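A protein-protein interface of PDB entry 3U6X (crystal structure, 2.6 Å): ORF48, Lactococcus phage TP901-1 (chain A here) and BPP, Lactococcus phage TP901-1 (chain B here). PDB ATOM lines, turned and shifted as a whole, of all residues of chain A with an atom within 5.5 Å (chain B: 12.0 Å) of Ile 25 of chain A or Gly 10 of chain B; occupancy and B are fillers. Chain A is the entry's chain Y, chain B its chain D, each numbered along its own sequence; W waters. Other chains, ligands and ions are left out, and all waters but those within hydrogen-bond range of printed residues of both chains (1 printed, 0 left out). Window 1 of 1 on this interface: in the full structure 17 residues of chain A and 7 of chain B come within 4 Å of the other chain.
The backbone NH (N) of Tyr 8 of chain B sits at hydrogen-bond distance from the side-chain sulfur (SD) of Met 11 of chain B (3.6 Å).
The backbone NH (N) of Val 87 of chain A is in hydrogen-bond range of the backbone carbonyl oxygen (O) of Tyr 21 of chain A.
The backbone carbonyl oxygen of Ala 24 of chain A lies within hydrogen-bond range of the side-chain hydroxyl of Thr 27 of chain A, at 2.7 Å.
The backbone NH (N) of Gly 26 of chain A sits at hydrogen-bond distance from the side-chain carboxylate (OE1) of Glu 28 of chain A.
The backbone carbonyl oxygen (O) of Gly 10 of chain B sits at hydrogen-bond distance from the side-chain hydroxyl (OH) of Tyr 21 of chain A.
The backbone NH of Gly 10 of chain B is in hydrogen-bond range of the backbone carbonyl oxygen of Ile 25 of chain A (2.8 Å).
N of Lys 12 of chain B sits at hydrogen-bond distance from OH of Tyr 21 of chain A (3.1 Å).
Tyr 21 of chain A touches Met 11 of chain B (OH to C, 3.6 Å).
Ala 24 of chain A touches Met 11 of chain B.
CA of Arg 9 of chain B touches O of Ile 25 of chain A, 3.3 Å away.
CE of Met 11 of chain B touches CG2 of Ile 25 of chain A, 3.9 Å away.
CD1 of Leu 80 of chain A touches CE2 of Tyr 8 of chain B, at 3.6 Å.
Arg 9 of chain B touches Leu 80 of chain A.
Leu 80 of chain A touches Gly 10 of chain B (CD1 to O, 3.4 Å).
Ile 82 of chain A touches Arg 9 of chain B (CD1 to O, 3.6 Å).
Ile 82 of chain A touches Gly 10 of chain B (CD1 to CA, 3.8 Å).
CG1 of Val 87 of chain A touches O of Gly 10 of chain B, at 3.4 Å.
Printed residues of chain B that touch a printed residue of chain A: Tyr 8, Arg 9, Gly 10, Met 11, Lys 12 and Ala 15.
Hydrophobic or aromatic side chains of chain B that line the printed part of chain A: Tyr 8, Met 11 and Ala 15.
Hydrophobic or aromatic side chains of chain A within 4 Å of the printed part of chain B: Tyr 21, Ala 24, Ile 25, Phe 38, Leu 80, Ile 82 and Val 87.
Among the printed residues, 18 pairs touch across the chains.
Among the printed residues, no Asp or Glu carboxylate lies within 4 Å of a Lys or Arg side-chain nitrogen of the other chain.
Water W1 lies within hydrogen-bond range of the side-chain carboxylate (OE2) of Glu 16 of chain B (2.8 Å), the backbone NH (N) of Ala 15 of chain B (2.8 Å), the backbone NH (N) of Gly 14 of chain B (2.9 Å) and the backbone carbonyl oxygen (O) of Gly 39 of chain A (3.0 Å).
Tyr 21 of chain A touches just these residues of chain B: Gly 10, Met 11 and Lys 12.
Of chain B, only Gly 10 and Met 11 come within 4 Å of Ala 24 of chain A.
Gly 26 of chain A touches just one residue of chain B: Arg 9.
Thr 27 of chain A touches just one residue of chain B: Gly 10 (3.6 Å).
No residue of chain B comes within 4 Å of Glu 28 of chain A.
Phe 38 of chain A touches just one residue of chain B: Ala 15.
No residue of chain B comes within 4 Å of Gly 39 of chain A.
No residue of chain B comes within 4 Å of Gly 40 of chain A.
Of the printed residues of chain B, Leu 80 of chain A touches Tyr 8, Arg 9 and Gly 10.
Printed residues of chain B within 4 Å of Ile 82 of chain A: Arg 9 (3.6 Å) and Gly 10 (3.8 Å).
Of chain B, only Gly 10 comes within 4 Å of Val 87 of chain A.
Of the printed residues of chain A, Arg 9 of chain B touches Ile 25, Gly 26, Leu 80 and Ile 82.
Printed residues of chain A within 4 Å of Gly 10 of chain B: Tyr 21 (2.8 Å), Ala 24 (3.8 Å), Ile 25 (2.8 Å), Thr 27 (3.6 Å), Leu 80 (3.4 Å), Ile 82 (3.8 Å) and Val 87 (3.4 Å).
Of the printed residues of chain A, Lys 12 of chain B touches Tyr 21 (3.1 Å).
Asn 13 of chain B touches none of the printed residues of chain A.
Of the printed residues of chain A, Ala 15 of chain B touches Phe 38 (3.5 Å).
Asp 20 of chain B touches none of the printed residues of chain A.
The nearest residue of chain B that does not touch Ile 25 of chain A is Ala 15 of chain B (4.2 Å).
The nearest residue of chain A that does not touch Gly 10 of chain B is Gly 26 of chain A (4.9 Å).
The nearest printed residue of chain B that does not touch Ile 82 of chain A is Met 11 of chain B (5.8 Å).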
ATOM      1  N   TYR A  21      29.011  -8.951  -6.954  1.00  0.00           N
ATOM      2  CA  TYR A  21      28.079  -8.437  -5.948  1.00  0.00           C
ATOM      3  C   TYR A  21      26.651  -8.398  -6.487  1.00  0.00           C
ATOM      4  O   TYR A  21      26.432  -8.340  -7.713  1.00  0.00           O
ATOM      5  CB  TYR A  21      28.490  -7.040  -5.445  1.00  0.00           C
ATOM      6  CG  TYR A  21      28.858  -6.078  -6.554  1.00  0.00           C
ATOM      7  CD1 TYR A  21      30.167  -5.977  -7.011  1.00  0.00           C
ATOM      8  CD2 TYR A  21      27.904  -5.235  -7.118  1.00  0.00           C
ATOM      9  CE1 TYR A  21      30.499  -5.120  -8.059  1.00  0.00           C
ATOM     10  CE2 TYR A  21      28.244  -4.330  -8.124  1.00  0.00           C
ATOM     11  CZ  TYR A  21      29.537  -4.287  -8.596  1.00  0.00           C
ATOM     12  OH  TYR A  21      29.853  -3.442  -9.618  1.00  0.00           O
ATOM     13  N   ASN A  23      22.577  -6.586  -5.831  1.00  0.00           N
ATOM     14  CA  ASN A  23      21.803  -5.405  -5.399  1.00  0.00           C
ATOM     15  C   ASN A  23      22.470  -4.037  -5.385  1.00  0.00           C
ATOM     16  O   ASN A  23      22.116  -3.161  -4.582  1.00  0.00           O
ATOM     17  CB  ASN A  23      21.043  -5.672  -4.094  1.00  0.00           C
ATOM     18  CG  ASN A  23      19.884  -6.608  -4.256  1.00  0.00           C
ATOM     19  OD1 ASN A  23      19.080  -6.513  -5.196  1.00  0.00           O
ATOM     20  ND2 ASN A  23      19.780  -7.549  -3.352  1.00  0.00           N
ATOM     21  N   ALA A  24      23.421  -3.830  -6.284  1.00  0.00           N
ATOM     22  CA  ALA A  24      24.065  -2.531  -6.440  1.00  0.00           C
ATOM     23  C   ALA A  24      22.998  -1.571  -6.987  1.00  0.00           C
ATOM     24  O   ALA A  24      22.026  -2.002  -7.593  1.00  0.00           O
ATOM     25  CB  ALA A  24      25.215  -2.641  -7.428  1.00  0.00           C
ATOM     26  N   ILE A  25      23.189  -0.290  -6.773  1.00  0.00           N
ATOM     27  CA  ILE A  25      22.353   0.817  -7.201  1.00  0.00           C
ATOM     28  C   ILE A  25      21.780   0.583  -8.623  1.00  0.00           C
ATOM     29  O   ILE A  25      22.527   0.309  -9.570  1.00  0.00           O
ATOM     30  CB  ILE A  25      23.226   2.093  -6.960  1.00  0.00           C
ATOM     31  CG1 ILE A  25      22.738   2.888  -5.779  1.00  0.00           C
ATOM     32  CG2 ILE A  25      23.593   2.973  -8.161  1.00  0.00           C
ATOM     33  CD1 ILE A  25      23.006   2.290  -4.492  1.00  0.00           C
ATOM     34  N   GLY A  26      20.456   0.501  -8.693  1.00  0.00           N
ATOM     35  CA  GLY A  26      19.734   0.311  -9.942  1.00  0.00           C
ATOM     36  C   GLY A  26      19.602  -1.111 -10.450  1.00  0.00           C
ATOM     37  O   GLY A  26      19.169  -1.307 -11.594  1.00  0.00           O
ATOM     38  N   THR A  27      20.010  -2.116  -9.625  1.00  0.00           N
ATOM     39  CA  THR A  27      19.880  -3.539  -9.971  1.00  0.00           C
ATOM     40  C   THR A  27      18.813  -4.221  -9.124  1.00  0.00           C
ATOM     41  O   THR A  27      18.461  -5.350  -9.405  1.00  0.00           O
ATOM     42  CB  THR A  27      21.219  -4.305  -9.959  1.00  0.00           C
ATOM     43  OG1 THR A  27      21.658  -4.453  -8.620  1.00  0.00           O
ATOM     44  CG2 THR A  27      22.284  -3.675 -10.843  1.00  0.00           C
ATOM     45  N   GLU A  28      18.286  -3.531  -8.104  1.00  0.00           N
ATOM     46  CA  GLU A  28      17.265  -4.067  -7.203  1.00  0.00           C
ATOM     47  C   GLU A  28      15.954  -4.355  -7.954  1.00  0.00           C
ATOM     48  O   GLU A  28      15.541  -3.580  -8.836  1.00  0.00           O
ATOM     49  CB  GLU A  28      17.021  -3.143  -5.996  1.00  0.00           C
ATOM     50  CG  GLU A  28      18.264  -2.524  -5.372  1.00  0.00           C
ATOM     51  CD  GLU A  28      18.600  -1.110  -5.825  1.00  0.00           C
ATOM     52  OE1 GLU A  28      18.527  -0.827  -7.049  1.00  0.00           O
ATOM     53  OE2 GLU A  28      18.946  -0.285  -4.944  1.00  0.00           O
ATOM     54  N   PHE A  32      14.984   1.384  -7.003  1.00  0.00           N
ATOM     55  CA  PHE A  32      15.993   2.030  -6.189  1.00  0.00           C
ATOM     56  C   PHE A  32      15.733   1.929  -4.698  1.00  0.00           C
ATOM     57  O   PHE A  32      14.636   2.229  -4.265  1.00  0.00           O
ATOM     58  CB  PHE A  32      16.131   3.495  -6.612  1.00  0.00           C
ATOM     59  CG  PHE A  32      17.327   4.191  -6.010  1.00  0.00           C
ATOM     60  CD1 PHE A  32      18.616   3.908  -6.458  1.00  0.00           C
ATOM     61  CD2 PHE A  32      17.172   5.113  -4.980  1.00  0.00           C
ATOM     62  CE1 PHE A  32      19.727   4.531  -5.874  1.00  0.00           C
ATOM     63  CE2 PHE A  32      18.288   5.717  -4.380  1.00  0.00           C
ATOM     64  CZ  PHE A  32      19.557   5.412  -4.823  1.00  0.00           C
ATOM     65  N   PHE A  38      21.195  -1.302   1.199  1.00  0.00           N
ATOM     66  CA  PHE A  38      21.370  -0.169   0.299  1.00  0.00           C
ATOM     67  C   PHE A  38      22.818  -0.046  -0.197  1.00  0.00           C
ATOM     68  O   PHE A  38      23.763  -0.049   0.598  1.00  0.00           O
ATOM     69  CB  PHE A  38      20.904   1.157   0.939  1.00  0.00           C
ATOM     70  CG  PHE A  38      21.156   2.336   0.018  1.00  0.00           C
ATOM     71  CD1 PHE A  38      20.406   2.505  -1.145  1.00  0.00           C
ATOM     72  CD2 PHE A  38      22.199   3.226   0.266  1.00  0.00           C
ATOM     73  CE1 PHE A  38      20.687   3.557  -2.034  1.00  0.00           C
ATOM     74  CE2 PHE A  38      22.486   4.266  -0.633  1.00  0.00           C
ATOM     75  CZ  PHE A  38      21.738   4.418  -1.779  1.00  0.00           C
ATOM     76  N   GLY A  39      22.966   0.024  -1.507  1.00  0.00           N
ATOM     77  CA  GLY A  39      24.263   0.163  -2.135  1.00  0.00           C
ATOM     78  C   GLY A  39      24.859  -1.117  -2.663  1.00  0.00           C
ATOM     79  O   GLY A  39      25.790  -1.062  -3.474  1.00  0.00           O
ATOM     80  N   GLY A  40      24.312  -2.251  -2.227  1.00  0.00           N
ATOM     81  CA  GLY A  40      24.778  -3.574  -2.622  1.00  0.00           C
ATOM     82  C   GLY A  40      25.143  -4.450  -1.439  1.00  0.00           C
ATOM     83  O   GLY A  40      25.504  -3.947  -0.360  1.00  0.00           O
ATOM     84  N   LEU A  80      30.961  -3.653 -16.860  1.00  0.00           N
ATOM     85  CA  LEU A  80      30.056  -4.420 -16.006  1.00  0.00           C
ATOM     86  C   LEU A  80      29.313  -5.424 -16.837  1.00  0.00           C
ATOM     87  O   LEU A  80      28.986  -5.161 -17.999  1.00  0.00           O
ATOM     88  CB  LEU A  80      28.989  -3.528 -15.336  1.00  0.00           C
ATOM     89  CG  LEU A  80      29.389  -2.403 -14.429  1.00  0.00           C
ATOM     90  CD1 LEU A  80      28.145  -1.695 -13.956  1.00  0.00           C
ATOM     91  CD2 LEU A  80      30.167  -2.918 -13.218  1.00  0.00           C
ATOM     92  N   ILE A  82      25.754  -7.227 -16.231  1.00  0.00           N
ATOM     93  CA  ILE A  82      24.589  -7.203 -15.320  1.00  0.00           C
ATOM     94  C   ILE A  82      23.522  -8.191 -15.732  1.00  0.00           C
ATOM     95  O   ILE A  82      23.053  -8.163 -16.874  1.00  0.00           O
ATOM     96  CB  ILE A  82      24.001  -5.774 -15.114  1.00  0.00           C
ATOM     97  CG1 ILE A  82      25.096  -4.715 -14.845  1.00  0.00           C
ATOM     98  CG2 ILE A  82      22.949  -5.795 -14.010  1.00  0.00           C
ATOM     99  CD1 ILE A  82      24.636  -3.274 -14.597  1.00  0.00           C
ATOM    100  N   VAL A  87      25.801  -8.563 -10.468  1.00  0.00           N
ATOM    101  CA  VAL A  87      26.803  -7.814 -11.222  1.00  0.00           C
ATOM    102  C   VAL A  87      28.190  -8.497 -11.122  1.00  0.00           C
ATOM    103  O   VAL A  87      28.585  -8.989 -10.053  1.00  0.00           O
ATOM    104  CB  VAL A  87      26.863  -6.313 -10.793  1.00  0.00           C
ATOM    105  CG1 VAL A  87      27.945  -5.550 -11.565  1.00  0.00           C
ATOM    106  CG2 VAL A  87      25.513  -5.629 -10.974  1.00  0.00           C
ATOM    107  N   LYS B   5      32.541  11.918  -9.492  1.00  0.00           N
ATOM    108  CA  LYS B   5      32.572  10.663 -10.237  1.00  0.00           C
ATOM    109  C   LYS B   5      31.163  10.288 -10.737  1.00  0.00           C
ATOM    110  O   LYS B   5      30.172  10.686 -10.111  1.00  0.00           O
ATOM    111  CB  LYS B   5      33.147   9.553  -9.369  1.00  0.00           C
ATOM    112  CG  LYS B   5      34.647   9.648  -9.188  1.00  0.00           C
ATOM    113  CD  LYS B   5      35.136   8.563  -8.248  1.00  0.00           C
ATOM    114  CE  LYS B   5      36.568   8.788  -7.829  1.00  0.00           C
ATOM    115  NZ  LYS B   5      36.661   9.542  -6.552  1.00  0.00           N
ATOM    116  N   LYS B   6      31.075   9.540 -11.881  1.00  0.00           N
ATOM    117  CA  LYS B   6      29.803   9.114 -12.482  1.00  0.00           C
ATOM    118  C   LYS B   6      29.069   8.155 -11.567  1.00  0.00           C
ATOM    119  O   LYS B   6      29.697   7.298 -10.941  1.00  0.00           O
ATOM    120  CB  LYS B   6      30.023   8.456 -13.850  1.00  0.00           C
ATOM    121  CG  LYS B   6      29.516   9.289 -15.012  1.00  0.00           C
ATOM    122  CD  LYS B   6      29.018   8.380 -16.145  1.00  0.00           C
ATOM    123  CE  LYS B   6      27.588   8.692 -16.539  1.00  0.00           C
ATOM    124  NZ  LYS B   6      27.444   9.047 -17.982  1.00  0.00           N
ATOM    125  N   VAL B   7      27.731   8.296 -11.497  1.00  0.00           N
ATOM    126  CA  VAL B   7      26.843   7.421 -10.743  1.00  0.00           C
ATOM    127  C   VAL B   7      26.053   6.639 -11.785  1.00  0.00           C
ATOM    128  O   VAL B   7      25.436   7.224 -12.673  1.00  0.00           O
ATOM    129  CB  VAL B   7      25.974   8.197  -9.733  1.00  0.00           C
ATOM    130  CG1 VAL B   7      24.865   7.319  -9.165  1.00  0.00           C
ATOM    131  CG2 VAL B   7      26.825   8.766  -8.606  1.00  0.00           C
ATOM    132  N   TYR B   8      26.134   5.311 -11.730  1.00  0.00           N
ATOM    133  CA  TYR B   8      25.501   4.460 -12.728  1.00  0.00           C
ATOM    134  C   TYR B   8      24.942   3.158 -12.172  1.00  0.00           C
ATOM    135  O   TYR B   8      25.377   2.705 -11.114  1.00  0.00           O
ATOM    136  CB  TYR B   8      26.487   4.192 -13.882  1.00  0.00           C
ATOM    137  CG  TYR B   8      27.796   3.589 -13.430  1.00  0.00           C
ATOM    138  CD1 TYR B   8      28.851   4.395 -13.020  1.00  0.00           C
ATOM    139  CD2 TYR B   8      27.990   2.213 -13.431  1.00  0.00           C
ATOM    140  CE1 TYR B   8      30.055   3.848 -12.581  1.00  0.00           C
ATOM    141  CE2 TYR B   8      29.201   1.654 -13.019  1.00  0.00           C
ATOM    142  CZ  TYR B   8      30.236   2.479 -12.604  1.00  0.00           C
ATOM    143  OH  TYR B   8      31.444   1.956 -12.207  1.00  0.00           O
ATOM    144  N   ARG B   9      23.983   2.552 -12.903  1.00  0.00           N
ATOM    145  CA  ARG B   9      23.369   1.265 -12.565  1.00  0.00           C
ATOM    146  C   ARG B   9      24.436   0.179 -12.499  1.00  0.00           C
ATOM    147  O   ARG B   9      25.248   0.054 -13.423  1.00  0.00           O
ATOM    148  CB  ARG B   9      22.327   0.919 -13.630  1.00  0.00           C
ATOM    149  CG  ARG B   9      21.688  -0.441 -13.515  1.00  0.00           C
ATOM    150  CD  ARG B   9      20.749  -0.679 -14.669  1.00  0.00           C
ATOM    151  NE  ARG B   9      20.409  -2.094 -14.800  1.00  0.00           N
ATOM    152  CZ  ARG B   9      20.708  -2.830 -15.860  1.00  0.00           C
ATOM    153  NH1 ARG B   9      21.360  -2.296 -16.884  1.00  0.00           N
ATOM    154  NH2 ARG B   9      20.361  -4.110 -15.906  1.00  0.00           N
ATOM    155  N   GLY B  10      24.442  -0.562 -11.391  1.00  0.00           N
ATOM    156  CA  GLY B  10      25.324  -1.703 -11.174  1.00  0.00           C
ATOM    157  C   GLY B  10      26.712  -1.390 -10.670  1.00  0.00           C
ATOM    158  O   GLY B  10      27.543  -2.291 -10.627  1.00  0.00           O
ATOM    159  N   MET B  11      26.996  -0.145 -10.277  1.00  0.00           N
ATOM    160  CA  MET B  11      28.321   0.190  -9.723  1.00  0.00           C
ATOM    161  C   MET B  11      28.506  -0.338  -8.305  1.00  0.00           C
ATOM    162  O   MET B  11      27.545  -0.303  -7.516  1.00  0.00           O
ATOM    163  CB  MET B  11      28.582   1.708  -9.728  1.00  0.00           C
ATOM    164  CG  MET B  11      27.703   2.534  -8.810  1.00  0.00           C
ATOM    165  SD  MET B  11      28.143   4.298  -8.889  1.00  0.00           S
ATOM    166  CE  MET B  11      26.914   4.917  -8.000  1.00  0.00           C
ATOM    167  N   LYS B  12      29.715  -0.826  -7.970  1.00  0.00           N
ATOM    168  CA  LYS B  12      29.962  -1.213  -6.593  1.00  0.00           C
ATOM    169  C   LYS B  12      30.296   0.095  -5.965  1.00  0.00           C
ATOM    170  O   LYS B  12      30.923   0.966  -6.626  1.00  0.00           O
ATOM    171  CB  LYS B  12      31.131  -2.217  -6.454  1.00  0.00           C
ATOM    172  CG  LYS B  12      32.542  -1.766  -6.825  1.00  0.00           C
ATOM    173  CD  LYS B  12      33.561  -2.483  -5.924  1.00  0.00           C
ATOM    174  CE  LYS B  12      34.975  -2.506  -6.453  1.00  0.00           C
ATOM    175  NZ  LYS B  12      35.096  -3.354  -7.660  1.00  0.00           N
ATOM    176  N   ASN B  13      29.923   0.279  -4.711  1.00  0.00           N
ATOM    177  CA  ASN B  13      30.244   1.580  -4.052  1.00  0.00           C
ATOM    178  C   ASN B  13      29.386   2.749  -4.526  1.00  0.00           C
ATOM    179  O   ASN B  13      29.871   3.877  -4.649  1.00  0.00           O
ATOM    180  CB  ASN B  13      31.753   1.944  -4.122  1.00  0.00           C
ATOM    181  CG  ASN B  13      32.642   0.856  -3.620  1.00  0.00           C
ATOM    182  OD1 ASN B  13      32.306   0.183  -2.651  1.00  0.00           O
ATOM    183  ND2 ASN B  13      33.765   0.630  -4.272  1.00  0.00           N
ATOM    184  N   GLY B  14      28.112   2.466  -4.759  1.00  0.00           N
ATOM    185  CA  GLY B  14      27.136   3.453  -5.170  1.00  0.00           C
ATOM    186  C   GLY B  14      26.843   4.433  -4.065  1.00  0.00           C
ATOM    187  O   GLY B  14      26.936   5.634  -4.283  1.00  0.00           O
ATOM    188  N   ALA B  15      26.527   3.929  -2.864  1.00  0.00           N
ATOM    189  CA  ALA B  15      26.279   4.714  -1.667  1.00  0.00           C
ATOM    190  C   ALA B  15      27.473   5.627  -1.349  1.00  0.00           C
ATOM    191  O   ALA B  15      27.291   6.843  -1.207  1.00  0.00           O
ATOM    192  CB  ALA B  15      25.987   3.778  -0.506  1.00  0.00           C
ATOM    193  N   GLU B  16      28.681   5.071  -1.320  1.00  0.00           N
ATOM    194  CA  GLU B  16      29.923   5.814  -1.079  1.00  0.00           C
ATOM    195  C   GLU B  16      30.243   6.845  -2.164  1.00  0.00           C
ATOM    196  O   GLU B  16      30.634   7.949  -1.805  1.00  0.00           O
ATOM    197  CB  GLU B  16      31.136   4.908  -0.708  1.00  0.00           C
ATOM    198  CG  GLU B  16      31.149   3.442  -1.106  1.00  0.00           C
ATOM    199  CD  GLU B  16      30.215   2.417  -0.469  1.00  0.00           C
ATOM    200  OE1 GLU B  16      30.716   1.385   0.024  1.00  0.00           O
ATOM    201  OE2 GLU B  16      28.982   2.586  -0.556  1.00  0.00           O
ATOM    202  N   THR B  17      30.007   6.541  -3.467  1.00  0.00           N
ATOM    203  CA  THR B  17      30.228   7.529  -4.552  1.00  0.00           C
ATOM    204  C   THR B  17      29.172   8.673  -4.525  1.00  0.00           C
ATOM    205  O   THR B  17      29.535   9.846  -4.713  1.00  0.00           O
ATOM    206  CB  THR B  17      30.412   6.849  -5.909  1.00  0.00           C
ATOM    207  OG1 THR B  17      31.454   5.867  -5.794  1.00  0.00           O
ATOM    208  CG2 THR B  17      30.736   7.828  -7.030  1.00  0.00           C
ATOM    209  N   ILE B  18      27.911   8.359  -4.214  1.00  0.00           N
ATOM    210  CA  ILE B  18      26.875   9.390  -4.072  1.00  0.00           C
ATOM    211  C   ILE B  18      27.280  10.311  -2.884  1.00  0.00           C
ATOM    212  O   ILE B  18      27.264  11.534  -3.022  1.00  0.00           O
ATOM    213  CB  ILE B  18      25.438   8.784  -3.893  1.00  0.00           C
ATOM    214  CG1 ILE B  18      24.974   7.955  -5.151  1.00  0.00           C
ATOM    215  CG2 ILE B  18      24.403   9.862  -3.500  1.00  0.00           C
ATOM    216  CD1 ILE B  18      23.829   6.987  -4.939  1.00  0.00           C
ATOM    217  N   ASN B  19      27.701   9.724  -1.748  1.00  0.00           N
ATOM    218  CA  ASN B  19      28.118  10.501  -0.583  1.00  0.00           C
ATOM    219  C   ASN B  19      29.299  11.403  -0.899  1.00  0.00           C
ATOM    220  O   ASN B  19      29.225  12.603  -0.646  1.00  0.00           O
ATOM    221  CB  ASN B  19      28.452   9.605   0.583  1.00  0.00           C
ATOM    222  CG  ASN B  19      28.712  10.370   1.847  1.00  0.00           C
ATOM    223  OD1 ASN B  19      27.808  10.841   2.509  1.00  0.00           O
ATOM    224  ND2 ASN B  19      29.947  10.556   2.190  1.00  0.00           N
ATOM    225  N   ASP B  20      30.366  10.845  -1.473  1.00  0.00           N
ATOM    226  CA  ASP B  20      31.556  11.590  -1.846  1.00  0.00           C
ATOM    227  C   ASP B  20      31.324  12.648  -2.938  1.00  0.00           C
ATOM    228  O   ASP B  20      32.038  13.647  -2.953  1.00  0.00           O
ATOM    229  CB  ASP B  20      32.711  10.630  -2.139  1.00  0.00           C
ATOM    230  CG  ASP B  20      33.209   9.834  -0.909  1.00  0.00           C
ATOM    231  OD1 ASP B  20      34.262   9.171  -1.021  1.00  0.00           O
ATOM    232  OD2 ASP B  20      32.556   9.908   0.178  1.00  0.00           O
ATOM    233  N   ASP B  21      30.283  12.483  -3.788  1.00  0.00           N
ATOM    234  CA  ASP B  21      29.935  13.484  -4.810  1.00  0.00           C
ATOM    235  C   ASP B  21      29.167  14.617  -4.152  1.00  0.00           C
ATOM    236  O   ASP B  21      29.434  15.785  -4.427  1.00  0.00           O
ATOM    237  CB  ASP B  21      29.105  12.880  -5.953  1.00  0.00           C
ATOM    238  CG  ASP B  21      29.886  12.031  -6.938  1.00  0.00           C
ATOM    239  OD1 ASP B  21      31.110  11.861  -6.737  1.00  0.00           O
ATOM    240  OD2 ASP B  21      29.266  11.522  -7.907  1.00  0.00           O
ATOM    241  N   LEU B  22      28.248  14.271  -3.239  1.00  0.00           N
ATOM    242  CA  LEU B  22      27.465  15.251  -2.490  1.00  0.00           C
ATOM    243  C   LEU B  22      28.379  16.119  -1.644  1.00  0.00           C
ATOM    244  O   LEU B  22      28.191  17.330  -1.610  1.00  0.00           O
ATOM    245  CB  LEU B  22      26.400  14.569  -1.611  1.00  0.00           C
ATOM    246  CG  LEU B  22      25.177  13.987  -2.314  1.00  0.00           C
ATOM    247  CD1 LEU B  22      24.415  13.062  -1.381  1.00  0.00           C
ATOM    248  CD2 LEU B  22      24.273  15.074  -2.813  1.00  0.00           C
HETATM  249  O   HOH W   1      27.287   1.247  -2.278  1.00  0.00           O
